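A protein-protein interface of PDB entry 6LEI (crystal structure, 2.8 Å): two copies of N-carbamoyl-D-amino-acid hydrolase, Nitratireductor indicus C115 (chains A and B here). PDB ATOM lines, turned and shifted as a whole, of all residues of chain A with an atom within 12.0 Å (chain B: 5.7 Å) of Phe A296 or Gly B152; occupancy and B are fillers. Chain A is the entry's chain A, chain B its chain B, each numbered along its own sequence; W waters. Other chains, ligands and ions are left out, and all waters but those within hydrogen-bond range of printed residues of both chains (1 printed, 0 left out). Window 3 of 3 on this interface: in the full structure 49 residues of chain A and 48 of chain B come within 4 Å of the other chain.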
ATOM      1  N   GLU A 178       9.762 -37.278  -7.176  1.00  0.00           N
ATOM      2  CA  GLU A 178       9.483 -36.637  -5.895  1.00  0.00           C
ATOM      3  C   GLU A 178      10.296 -37.263  -4.770  1.00  0.00           C
ATOM      4  O   GLU A 178      10.615 -36.588  -3.786  1.00  0.00           O
ATOM      5  CB  GLU A 178       7.990 -36.718  -5.575  1.00  0.00           C
ATOM      6  CG  GLU A 178       7.087 -35.935  -6.520  1.00  0.00           C
ATOM      7  CD  GLU A 178       6.684 -36.729  -7.751  1.00  0.00           C
ATOM      8  OE1 GLU A 178       7.269 -37.807  -7.990  1.00  0.00           O
ATOM      9  OE2 GLU A 178       5.774 -36.275  -8.477  1.00  0.00           O
ATOM     10  N   ARG A 181      13.724 -35.462  -5.005  1.00  0.00           N
ATOM     11  CA  ARG A 181      13.677 -34.010  -4.851  1.00  0.00           C
ATOM     12  C   ARG A 181      13.362 -33.604  -3.417  1.00  0.00           C
ATOM     13  O   ARG A 181      13.976 -32.671  -2.885  1.00  0.00           O
ATOM     14  CB  ARG A 181      12.647 -33.411  -5.807  1.00  0.00           C
ATOM     15  CG  ARG A 181      12.543 -31.898  -5.711  1.00  0.00           C
ATOM     16  CD  ARG A 181      13.053 -31.229  -6.975  1.00  0.00           C
ATOM     17  NE  ARG A 181      14.373 -31.714  -7.363  1.00  0.00           N
ATOM     18  CZ  ARG A 181      14.993 -31.370  -8.487  1.00  0.00           C
ATOM     19  NH1 ARG A 181      14.415 -30.534  -9.339  1.00  0.00           N
ATOM     20  NH2 ARG A 181      16.194 -31.862  -8.760  1.00  0.00           N
ATOM     21  N   PHE A 288      19.681 -24.973  -6.054  1.00  0.00           N
ATOM     22  CA  PHE A 288      18.224 -24.996  -5.979  1.00  0.00           C
ATOM     23  C   PHE A 288      17.664 -23.621  -5.635  1.00  0.00           C
ATOM     24  O   PHE A 288      16.607 -23.231  -6.142  1.00  0.00           O
ATOM     25  CB  PHE A 288      17.767 -26.037  -4.957  1.00  0.00           C
ATOM     26  CG  PHE A 288      17.892 -27.457  -5.436  1.00  0.00           C
ATOM     27  CD1 PHE A 288      18.224 -27.734  -6.753  1.00  0.00           C
ATOM     28  CD2 PHE A 288      17.664 -28.516  -4.574  1.00  0.00           C
ATOM     29  CE1 PHE A 288      18.335 -29.039  -7.196  1.00  0.00           C
ATOM     30  CE2 PHE A 288      17.773 -29.824  -5.011  1.00  0.00           C
ATOM     31  CZ  PHE A 288      18.109 -30.085  -6.324  1.00  0.00           C
ATOM     32  N   ALA A 290      18.748 -20.770  -6.525  1.00  0.00           N
ATOM     33  CA  ALA A 290      19.015 -19.778  -7.558  1.00  0.00           C
ATOM     34  C   ALA A 290      18.085 -19.900  -8.760  1.00  0.00           C
ATOM     35  O   ALA A 290      17.563 -18.891  -9.243  1.00  0.00           O
ATOM     36  CB  ALA A 290      20.473 -19.881  -8.019  1.00  0.00           C
ATOM     37  N   HIS A 291      17.863 -21.117  -9.255  1.00  0.00           N
ATOM     38  CA  HIS A 291      17.142 -21.307 -10.507  1.00  0.00           C
ATOM     39  C   HIS A 291      15.704 -21.769 -10.326  1.00  0.00           C
ATOM     40  O   HIS A 291      14.862 -21.473 -11.180  1.00  0.00           O
ATOM     41  CB  HIS A 291      17.877 -22.318 -11.393  1.00  0.00           C
ATOM     42  CG  HIS A 291      19.352 -22.078 -11.494  1.00  0.00           C
ATOM     43  ND1 HIS A 291      19.890 -21.068 -12.260  1.00  0.00           N
ATOM     44  CD2 HIS A 291      20.400 -22.720 -10.928  1.00  0.00           C
ATOM     45  CE1 HIS A 291      21.207 -21.096 -12.160  1.00  0.00           C
ATOM     46  NE2 HIS A 291      21.543 -22.090 -11.358  1.00  0.00           N
ATOM     47  N   ARG A 292      15.397 -22.487  -9.247  1.00  0.00           N
ATOM     48  CA  ARG A 292      14.071 -23.071  -9.093  1.00  0.00           C
ATOM     49  C   ARG A 292      13.007 -21.990  -8.941  1.00  0.00           C
ATOM     50  O   ARG A 292      13.185 -21.016  -8.204  1.00  0.00           O
ATOM     51  CB  ARG A 292      14.034 -24.014  -7.889  1.00  0.00           C
ATOM     52  CG  ARG A 292      14.912 -25.248  -8.040  1.00  0.00           C
ATOM     53  CD  ARG A 292      14.725 -26.223  -6.885  1.00  0.00           C
ATOM     54  NE  ARG A 292      13.448 -26.930  -6.949  1.00  0.00           N
ATOM     55  CZ  ARG A 292      12.373 -26.605  -6.239  1.00  0.00           C
ATOM     56  NH1 ARG A 292      12.413 -25.580  -5.398  1.00  0.00           N
ATOM     57  NH2 ARG A 292      11.257 -27.310  -6.365  1.00  0.00           N
ATOM     58  N   ARG A 293      11.893 -22.171  -9.652  1.00  0.00           N
ATOM     59  CA  ARG A 293      10.742 -21.271  -9.603  1.00  0.00           C
ATOM     60  C   ARG A 293       9.550 -22.073  -9.103  1.00  0.00           C
ATOM     61  O   ARG A 293       8.798 -22.651  -9.903  1.00  0.00           O
ATOM     62  CB  ARG A 293      10.460 -20.660 -10.975  1.00  0.00           C
ATOM     63  CG  ARG A 293      11.685 -20.088 -11.673  1.00  0.00           C
ATOM     64  CD  ARG A 293      12.235 -18.878 -10.941  1.00  0.00           C
ATOM     65  NE  ARG A 293      11.251 -17.804 -10.846  1.00  0.00           N
ATOM     66  CZ  ARG A 293      11.518 -16.585 -10.391  1.00  0.00           C
ATOM     67  NH1 ARG A 293      12.744 -16.278  -9.992  1.00  0.00           N
ATOM     68  NH2 ARG A 293      10.559 -15.670 -10.340  1.00  0.00           N
ATOM     69  N   PRO A 294       9.334 -22.136  -7.785  1.00  0.00           N
ATOM     70  CA  PRO A 294       8.266 -22.997  -7.250  1.00  0.00           C
ATOM     71  C   PRO A 294       6.859 -22.522  -7.577  1.00  0.00           C
ATOM     72  O   PRO A 294       5.906 -23.270  -7.324  1.00  0.00           O
ATOM     73  CB  PRO A 294       8.520 -22.971  -5.739  1.00  0.00           C
ATOM     74  CG  PRO A 294       9.219 -21.674  -5.502  1.00  0.00           C
ATOM     75  CD  PRO A 294      10.075 -21.444  -6.717  1.00  0.00           C
ATOM     76  N   GLU A 295       6.692 -21.317  -8.123  1.00  0.00           N
ATOM     77  CA  GLU A 295       5.355 -20.841  -8.458  1.00  0.00           C
ATOM     78  C   GLU A 295       4.785 -21.512  -9.703  1.00  0.00           C
ATOM     79  O   GLU A 295       3.594 -21.340  -9.985  1.00  0.00           O
ATOM     80  CB  GLU A 295       5.361 -19.320  -8.642  1.00  0.00           C
ATOM     81  CG  GLU A 295       6.222 -18.811  -9.792  1.00  0.00           C
ATOM     82  CD  GLU A 295       7.688 -18.675  -9.424  1.00  0.00           C
ATOM     83  OE1 GLU A 295       8.074 -19.112  -8.318  1.00  0.00           O
ATOM     84  OE2 GLU A 295       8.457 -18.126 -10.241  1.00  0.00           O
ATOM     85  N   PHE A 296       5.593 -22.268 -10.444  1.00  0.00           N
ATOM     86  CA  PHE A 296       5.125 -22.997 -11.614  1.00  0.00           C
ATOM     87  C   PHE A 296       5.026 -24.498 -11.378  1.00  0.00           C
ATOM     88  O   PHE A 296       4.700 -25.237 -12.314  1.00  0.00           O
ATOM     89  CB  PHE A 296       6.043 -22.728 -12.812  1.00  0.00           C
ATOM     90  CG  PHE A 296       6.027 -21.302 -13.281  1.00  0.00           C
ATOM     91  CD1 PHE A 296       5.049 -20.858 -14.156  1.00  0.00           C
ATOM     92  CD2 PHE A 296       6.991 -20.407 -12.852  1.00  0.00           C
ATOM     93  CE1 PHE A 296       5.032 -19.545 -14.591  1.00  0.00           C
ATOM     94  CE2 PHE A 296       6.981 -19.093 -13.284  1.00  0.00           C
ATOM     95  CZ  PHE A 296       5.998 -18.662 -14.154  1.00  0.00           C
ATOM     96  N   TYR A 297       5.294 -24.969 -10.159  1.00  0.00           N
ATOM     97  CA  TYR A 297       5.281 -26.393  -9.847  1.00  0.00           C
ATOM     98  C   TYR A 297       4.054 -26.796  -9.035  1.00  0.00           C
ATOM     99  O   TYR A 297       4.032 -27.888  -8.459  1.00  0.00           O
ATOM    100  CB  TYR A 297       6.549 -26.791  -9.088  1.00  0.00           C
ATOM    101  CG  TYR A 297       7.855 -26.296  -9.675  1.00  0.00           C
ATOM    102  CD1 TYR A 297       7.997 -26.065 -11.039  1.00  0.00           C
ATOM    103  CD2 TYR A 297       8.955 -26.067  -8.857  1.00  0.00           C
ATOM    104  CE1 TYR A 297       9.194 -25.614 -11.566  1.00  0.00           C
ATOM    105  CE2 TYR A 297      10.153 -25.616  -9.374  1.00  0.00           C
ATOM    106  CZ  TYR A 297      10.268 -25.392 -10.727  1.00  0.00           C
ATOM    107  OH  TYR A 297      11.464 -24.944 -11.240  1.00  0.00           O
ATOM    108  N   GLN A 298       3.030 -25.938  -8.984  1.00  0.00           N
ATOM    109  CA  GLN A 298       1.926 -26.154  -8.053  1.00  0.00           C
ATOM    110  C   GLN A 298       1.140 -27.421  -8.368  1.00  0.00           C
ATOM    111  O   GLN A 298       0.527 -28.004  -7.466  1.00  0.00           O
ATOM    112  CB  GLN A 298       0.996 -24.940  -8.052  1.00  0.00           C
ATOM    113  CG  GLN A 298       1.602 -23.703  -7.411  1.00  0.00           C
ATOM    114  CD  GLN A 298       1.948 -23.915  -5.948  1.00  0.00           C
ATOM    115  OE1 GLN A 298       1.285 -24.677  -5.243  1.00  0.00           O
ATOM    116  NE2 GLN A 298       2.996 -23.243  -5.486  1.00  0.00           N
ATOM    117  N   ARG A 299       1.145 -27.865  -9.626  1.00  0.00           N
ATOM    118  CA  ARG A 299       0.435 -29.090  -9.978  1.00  0.00           C
ATOM    119  C   ARG A 299       1.012 -30.314  -9.278  1.00  0.00           C
ATOM    120  O   ARG A 299       0.293 -31.301  -9.091  1.00  0.00           O
ATOM    121  CB  ARG A 299       0.460 -29.301 -11.493  1.00  0.00           C
ATOM    122  CG  ARG A 299      -0.370 -28.300 -12.277  1.00  0.00           C
ATOM    123  CD  ARG A 299      -0.323 -28.601 -13.764  1.00  0.00           C
ATOM    124  NE  ARG A 299      -1.196 -27.718 -14.531  1.00  0.00           N
ATOM    125  CZ  ARG A 299      -2.466 -27.988 -14.817  1.00  0.00           C
ATOM    126  NH1 ARG A 299      -3.186 -27.128 -15.523  1.00  0.00           N
ATOM    127  NH2 ARG A 299      -3.015 -29.120 -14.398  1.00  0.00           N
ATOM    128  N   ILE A 300       2.286 -30.268  -8.882  1.00  0.00           N
ATOM    129  CA  ILE A 300       2.908 -31.416  -8.232  1.00  0.00           C
ATOM    130  C   ILE A 300       2.275 -31.684  -6.871  1.00  0.00           C
ATOM    131  O   ILE A 300       2.211 -32.837  -6.425  1.00  0.00           O
ATOM    132  CB  ILE A 300       4.430 -31.195  -8.124  1.00  0.00           C
ATOM    133  CG1 ILE A 300       5.025 -30.949  -9.512  1.00  0.00           C
ATOM    134  CG2 ILE A 300       5.109 -32.384  -7.461  1.00  0.00           C
ATOM    135  CD1 ILE A 300       6.526 -30.771  -9.515  1.00  0.00           C
ATOM    136  N   THR A 301       1.781 -30.642  -6.199  1.00  0.00           N
ATOM    137  CA  THR A 301       1.161 -30.796  -4.890  1.00  0.00           C
ATOM    138  C   THR A 301      -0.337 -30.532  -4.880  1.00  0.00           C
ATOM    139  O   THR A 301      -1.001 -30.901  -3.906  1.00  0.00           O
ATOM    140  CB  THR A 301       1.829 -29.864  -3.867  1.00  0.00           C
ATOM    141  OG1 THR A 301       1.767 -28.513  -4.338  1.00  0.00           O
ATOM    142  CG2 THR A 301       3.282 -30.258  -3.658  1.00  0.00           C
ATOM    143  N   SER A 302      -0.884 -29.912  -5.926  1.00  0.00           N
ATOM    144  CA  SER A 302      -2.312 -29.611  -5.942  1.00  0.00           C
ATOM    145  C   SER A 302      -3.142 -30.834  -6.310  1.00  0.00           C
ATOM    146  O   SER A 302      -4.219 -31.048  -5.742  1.00  0.00           O
ATOM    147  CB  SER A 302      -2.600 -28.468  -6.917  1.00  0.00           C
ATOM    148  OG  SER A 302      -1.957 -27.274  -6.508  1.00  0.00           O
ATOM    149  N   GLN A 303      -2.664 -31.644  -7.250  1.00  0.00           N
ATOM    150  CA  GLN A 303      -3.405 -32.793  -7.741  1.00  0.00           C
ATOM    151  C   GLN A 303      -2.581 -34.063  -7.578  1.00  0.00           C
ATOM    152  O   GLN A 303      -1.359 -34.022  -7.412  1.00  0.00           O
ATOM    153  CB  GLN A 303      -3.801 -32.605  -9.212  1.00  0.00           C
ATOM    154  CG  GLN A 303      -2.629 -32.327 -10.140  1.00  0.00           C
ATOM    155  CD  GLN A 303      -3.070 -31.897 -11.525  1.00  0.00           C
ATOM    156  OE1 GLN A 303      -3.457 -30.748 -11.737  1.00  0.00           O
ATOM    157  NE2 GLN A 303      -3.012 -32.820 -12.478  1.00  0.00           N
ATOM    158  N   GLU A 307      -5.400 -34.088 -14.637  1.00  0.00           N
ATOM    159  CA  GLU A 307      -6.660 -33.354 -14.574  1.00  0.00           C
ATOM    160  C   GLU A 307      -7.486 -33.583 -15.834  1.00  0.00           C
ATOM    161  O   GLU A 307      -8.671 -33.902 -15.759  1.00  0.00           O
ATOM    162  CB  GLU A 307      -6.414 -31.856 -14.374  1.00  0.00           C
ATOM    163  CG  GLU A 307      -5.719 -31.168 -15.537  1.00  0.00           C
ATOM    164  CD  GLU A 307      -6.046 -29.688 -15.613  1.00  0.00           C
ATOM    165  OE1 GLU A 307      -6.891 -29.307 -16.450  1.00  0.00           O
ATOM    166  OE2 GLU A 307      -5.469 -28.908 -14.826  1.00  0.00           O
ATOM    167  N   PHE B 108      10.879 -12.147 -23.691  1.00  0.00           N
ATOM    168  CA  PHE B 108      10.812 -13.530 -23.247  1.00  0.00           C
ATOM    169  C   PHE B 108      11.624 -14.421 -24.174  1.00  0.00           C
ATOM    170  O   PHE B 108      11.824 -14.107 -25.351  1.00  0.00           O
ATOM    171  CB  PHE B 108       9.364 -14.046 -23.203  1.00  0.00           C
ATOM    172  CG  PHE B 108       8.467 -13.278 -22.276  1.00  0.00           C
ATOM    173  CD1 PHE B 108       8.502 -13.506 -20.912  1.00  0.00           C
ATOM    174  CD2 PHE B 108       7.576 -12.341 -22.773  1.00  0.00           C
ATOM    175  CE1 PHE B 108       7.672 -12.805 -20.056  1.00  0.00           C
ATOM    176  CE2 PHE B 108       6.744 -11.637 -21.923  1.00  0.00           C
ATOM    177  CZ  PHE B 108       6.793 -11.870 -20.563  1.00  0.00           C
ATOM    178  N   ARG B 125       6.723 -19.706 -22.739  1.00  0.00           N
ATOM    179  CA  ARG B 125       7.779 -18.748 -22.450  1.00  0.00           C
ATOM    180  C   ARG B 125       8.664 -19.291 -21.339  1.00  0.00           C
ATOM    181  O   ARG B 125       8.169 -19.835 -20.346  1.00  0.00           O
ATOM    182  CB  ARG B 125       7.190 -17.386 -22.069  1.00  0.00           C
ATOM    183  CG  ARG B 125       6.443 -16.731 -23.221  1.00  0.00           C
ATOM    184  CD  ARG B 125       5.716 -15.466 -22.809  1.00  0.00           C
ATOM    185  NE  ARG B 125       5.078 -14.831 -23.960  1.00  0.00           N
ATOM    186  CZ  ARG B 125       4.270 -13.780 -23.888  1.00  0.00           C
ATOM    187  NH1 ARG B 125       3.988 -13.235 -22.713  1.00  0.00           N
ATOM    188  NH2 ARG B 125       3.739 -13.275 -24.993  1.00  0.00           N
ATOM    189  N   LYS B 126       9.975 -19.137 -21.519  1.00  0.00           N
ATOM    190  CA  LYS B 126      10.949 -19.811 -20.668  1.00  0.00           C
ATOM    191  C   LYS B 126      10.777 -19.412 -19.209  1.00  0.00           C
ATOM    192  O   LYS B 126      10.537 -18.245 -18.887  1.00  0.00           O
ATOM    193  CB  LYS B 126      12.365 -19.486 -21.143  1.00  0.00           C
ATOM    194  CG  LYS B 126      13.445 -20.385 -20.572  1.00  0.00           C
ATOM    195  CD  LYS B 126      14.782 -20.106 -21.237  1.00  0.00           C
ATOM    196  CE  LYS B 126      15.831 -21.113 -20.810  1.00  0.00           C
ATOM    197  NZ  LYS B 126      17.129 -20.890 -21.504  1.00  0.00           N
ATOM    198  N   ILE B 127      10.905 -20.397 -18.321  1.00  0.00           N
ATOM    199  CA  ILE B 127      10.691 -20.185 -16.894  1.00  0.00           C
ATOM    200  C   ILE B 127      12.029 -20.105 -16.171  1.00  0.00           C
ATOM    201  O   ILE B 127      12.309 -19.128 -15.467  1.00  0.00           O
ATOM    202  CB  ILE B 127       9.805 -21.299 -16.307  1.00  0.00           C
ATOM    203  CG1 ILE B 127       8.385 -21.200 -16.863  1.00  0.00           C
ATOM    204  CG2 ILE B 127       9.811 -21.241 -14.790  1.00  0.00           C
ATOM    205  CD1 ILE B 127       7.463 -22.313 -16.407  1.00  0.00           C
ATOM    206  N   GLU B 150      12.972 -11.929 -19.427  1.00  0.00           N
ATOM    207  CA  GLU B 150      12.184 -11.967 -18.207  1.00  0.00           C
ATOM    208  C   GLU B 150      11.630 -13.372 -18.004  1.00  0.00           C
ATOM    209  O   GLU B 150      11.549 -14.171 -18.940  1.00  0.00           O
ATOM    210  CB  GLU B 150      11.036 -10.953 -18.259  1.00  0.00           C
ATOM    211  CG  GLU B 150      11.457  -9.552 -18.667  1.00  0.00           C
ATOM    212  CD  GLU B 150      10.278  -8.609 -18.802  1.00  0.00           C
ATOM    213  OE1 GLU B 150       9.194  -8.932 -18.270  1.00  0.00           O
ATOM    214  OE2 GLU B 150      10.433  -7.548 -19.444  1.00  0.00           O
ATOM    215  N   VAL B 151      11.251 -13.668 -16.762  1.00  0.00           N
ATOM    216  CA  VAL B 151      10.660 -14.965 -16.457  1.00  0.00           C
ATOM    217  C   VAL B 151       9.317 -15.079 -17.164  1.00  0.00           C
ATOM    218  O   VAL B 151       8.490 -14.159 -17.114  1.00  0.00           O
ATOM    219  CB  VAL B 151      10.515 -15.149 -14.938  1.00  0.00           C
ATOM    220  CG1 VAL B 151       9.865 -16.489 -14.626  1.00  0.00           C
ATOM    221  CG2 VAL B 151      11.872 -15.044 -14.262  1.00  0.00           C
ATOM    222  N   GLY B 152       9.100 -16.207 -17.838  1.00  0.00           N
ATOM    223  CA  GLY B 152       7.876 -16.393 -18.590  1.00  0.00           C
ATOM    224  C   GLY B 152       6.644 -16.384 -17.706  1.00  0.00           C
ATOM    225  O   GLY B 152       6.696 -16.643 -16.502  1.00  0.00           O
ATOM    226  N   ASN B 153       5.507 -16.072 -18.331  1.00  0.00           N
ATOM    227  CA  ASN B 153       4.228 -15.984 -17.635  1.00  0.00           C
ATOM    228  C   ASN B 153       3.188 -16.931 -18.223  1.00  0.00           C
ATOM    229  O   ASN B 153       1.985 -16.696 -18.072  1.00  0.00           O
ATOM    230  CB  ASN B 153       3.705 -14.548 -17.656  1.00  0.00           C
ATOM    231  CG  ASN B 153       3.769 -13.924 -19.037  1.00  0.00           C
ATOM    232  OD1 ASN B 153       4.036 -14.605 -20.029  1.00  0.00           O
ATOM    233  ND2 ASN B 153       3.524 -12.621 -19.108  1.00  0.00           N
ATOM    234  N   THR B 154       3.624 -17.997 -18.890  1.00  0.00           N
ATOM    235  CA  THR B 154       2.704 -18.963 -19.476  1.00  0.00           C
ATOM    236  C   THR B 154       2.606 -20.257 -18.688  1.00  0.00           C
ATOM    237  O   THR B 154       1.549 -20.896 -18.699  1.00  0.00           O
ATOM    238  CB  THR B 154       3.120 -19.300 -20.912  1.00  0.00           C
ATOM    239  OG1 THR B 154       4.378 -19.989 -20.892  1.00  0.00           O
ATOM    240  CG2 THR B 154       3.254 -18.032 -21.735  1.00  0.00           C
ATOM    241  N   GLY B 155       3.673 -20.651 -18.001  1.00  0.00           N
ATOM    242  CA  GLY B 155       3.712 -21.927 -17.326  1.00  0.00           C
ATOM    243  C   GLY B 155       3.906 -23.062 -18.313  1.00  0.00           C
ATOM    244  O   GLY B 155       3.878 -22.887 -19.533  1.00  0.00           O
ATOM    245  N   PHE B 156       4.120 -24.255 -17.767  1.00  0.00           N
ATOM    246  CA  PHE B 156       4.296 -25.457 -18.578  1.00  0.00           C
ATOM    247  C   PHE B 156       2.921 -25.913 -19.045  1.00  0.00           C
ATOM    248  O   PHE B 156       2.257 -26.727 -18.404  1.00  0.00           O
ATOM    249  CB  PHE B 156       5.022 -26.543 -17.791  1.00  0.00           C
ATOM    250  CG  PHE B 156       6.465 -26.229 -17.517  1.00  0.00           C
ATOM    251  CD1 PHE B 156       7.365 -26.106 -18.561  1.00  0.00           C
ATOM    252  CD2 PHE B 156       6.925 -26.070 -16.220  1.00  0.00           C
ATOM    253  CE1 PHE B 156       8.691 -25.816 -18.322  1.00  0.00           C
ATOM    254  CE2 PHE B 156       8.256 -25.782 -15.972  1.00  0.00           C
ATOM    255  CZ  PHE B 156       9.139 -25.655 -17.026  1.00  0.00           C
ATOM    256  N   VAL B 182       5.260 -31.526 -14.214  1.00  0.00           N
ATOM    257  CA  VAL B 182       4.148 -30.584 -14.323  1.00  0.00           C
ATOM    258  C   VAL B 182       3.339 -30.862 -15.584  1.00  0.00           C
ATOM    259  O   VAL B 182       2.105 -30.918 -15.553  1.00  0.00           O
ATOM    260  CB  VAL B 182       4.663 -29.133 -14.288  1.00  0.00           C
ATOM    261  CG1 VAL B 182       3.607 -28.181 -14.826  1.00  0.00           C
ATOM    262  CG2 VAL B 182       5.049 -28.746 -12.869  1.00  0.00           C
HETATM  263  O   HOH W   1       3.800 -24.279 -14.815  1.00  0.00           O
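The side-chain hydroxyl (OH) of Tyr A297 is in hydrogen-bond range of the backbone NH (N) of Arg A293 (3.2 Å). The backbone NH (N) of Gly B152 lies within hydrogen-bond range of the backbone carbonyl oxygen (O) of Lys B126 (2.7 Å). NH2 of Arg A299 is in hydrogen-bond range of OE1 of Gln A303 (3.2 Å). The side-chain carboxylate of Glu A307 is in salt-bridge range of the guanidinium group of Arg A299, 2.5 Å away. The side-chain carboxylate (OE2) of Glu A295 is in salt-bridge range of the guanidinium group (NE) of Arg A293.
Among the printed residues, merely in contact across the chains: Phe A296 with Gly B152 (3.2 Å), Phe A296 with Ile B127 (3.5 Å), Phe A296 with Val B182 (3.6 Å), Phe A296 with Gly B155 (3.6 Å), Arg A299 with Val B182 (3.8 Å), Arg A293 with Ile B127 (3.8 Å) and Tyr A297 with Val B182 (3.8 Å).
Printed residues of chain B within 4 Å of Arg A293: Ile B127. Phe A296 touches four residues of chain B. Of the printed residues of chain B, Tyr A297 touches Val B182 (3.8 Å). Of the printed residues of chain B, Arg A299 touches Val B182 (3.8 Å). Thr A301 touches none of the printed residues of chain B. No residue of chain A comes within 4 Å of Val B151. Of chain A, only Phe A296 comes within 4 Å of Gly B152. No residue of chain A comes within 4 Å of Thr B154. Of the printed residues of chain A, Val B182 touches Phe A296, Tyr A297 and Arg A299. The nearest residue of chain B that does not touch Phe A296 is Val B151 (4.1 Å). The nearest printed residue of chain B that does not touch Arg A293 is Val B151 (4.2 Å).
Of the 18 printed residues of chain A, 4 touch a printed residue of chain B. Of the 12 printed residues of chain B, 4 touch a printed residue of chain A. Printed residues of chain B that touch a printed residue of chain A: Ile B127, Gly B152, Gly B155 and Val B182. Hydrophobic or aromatic side chains of chain B that line the printed part of chain A: Ile B127 and Val B182. Among the printed residues, no Asp or Glu carboxylate lies within 4 Å of a Lys or Arg side-chain nitrogen of the other chain.
No position is printed for both chains. Of the 7 pairs that touch across the chains among the printed residues, none has its exchanged pair printed and touching as well.
Water W1 lies within hydrogen-bond range of the backbone carbonyl oxygen of Phe A296 and the backbone NH of Phe B156.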
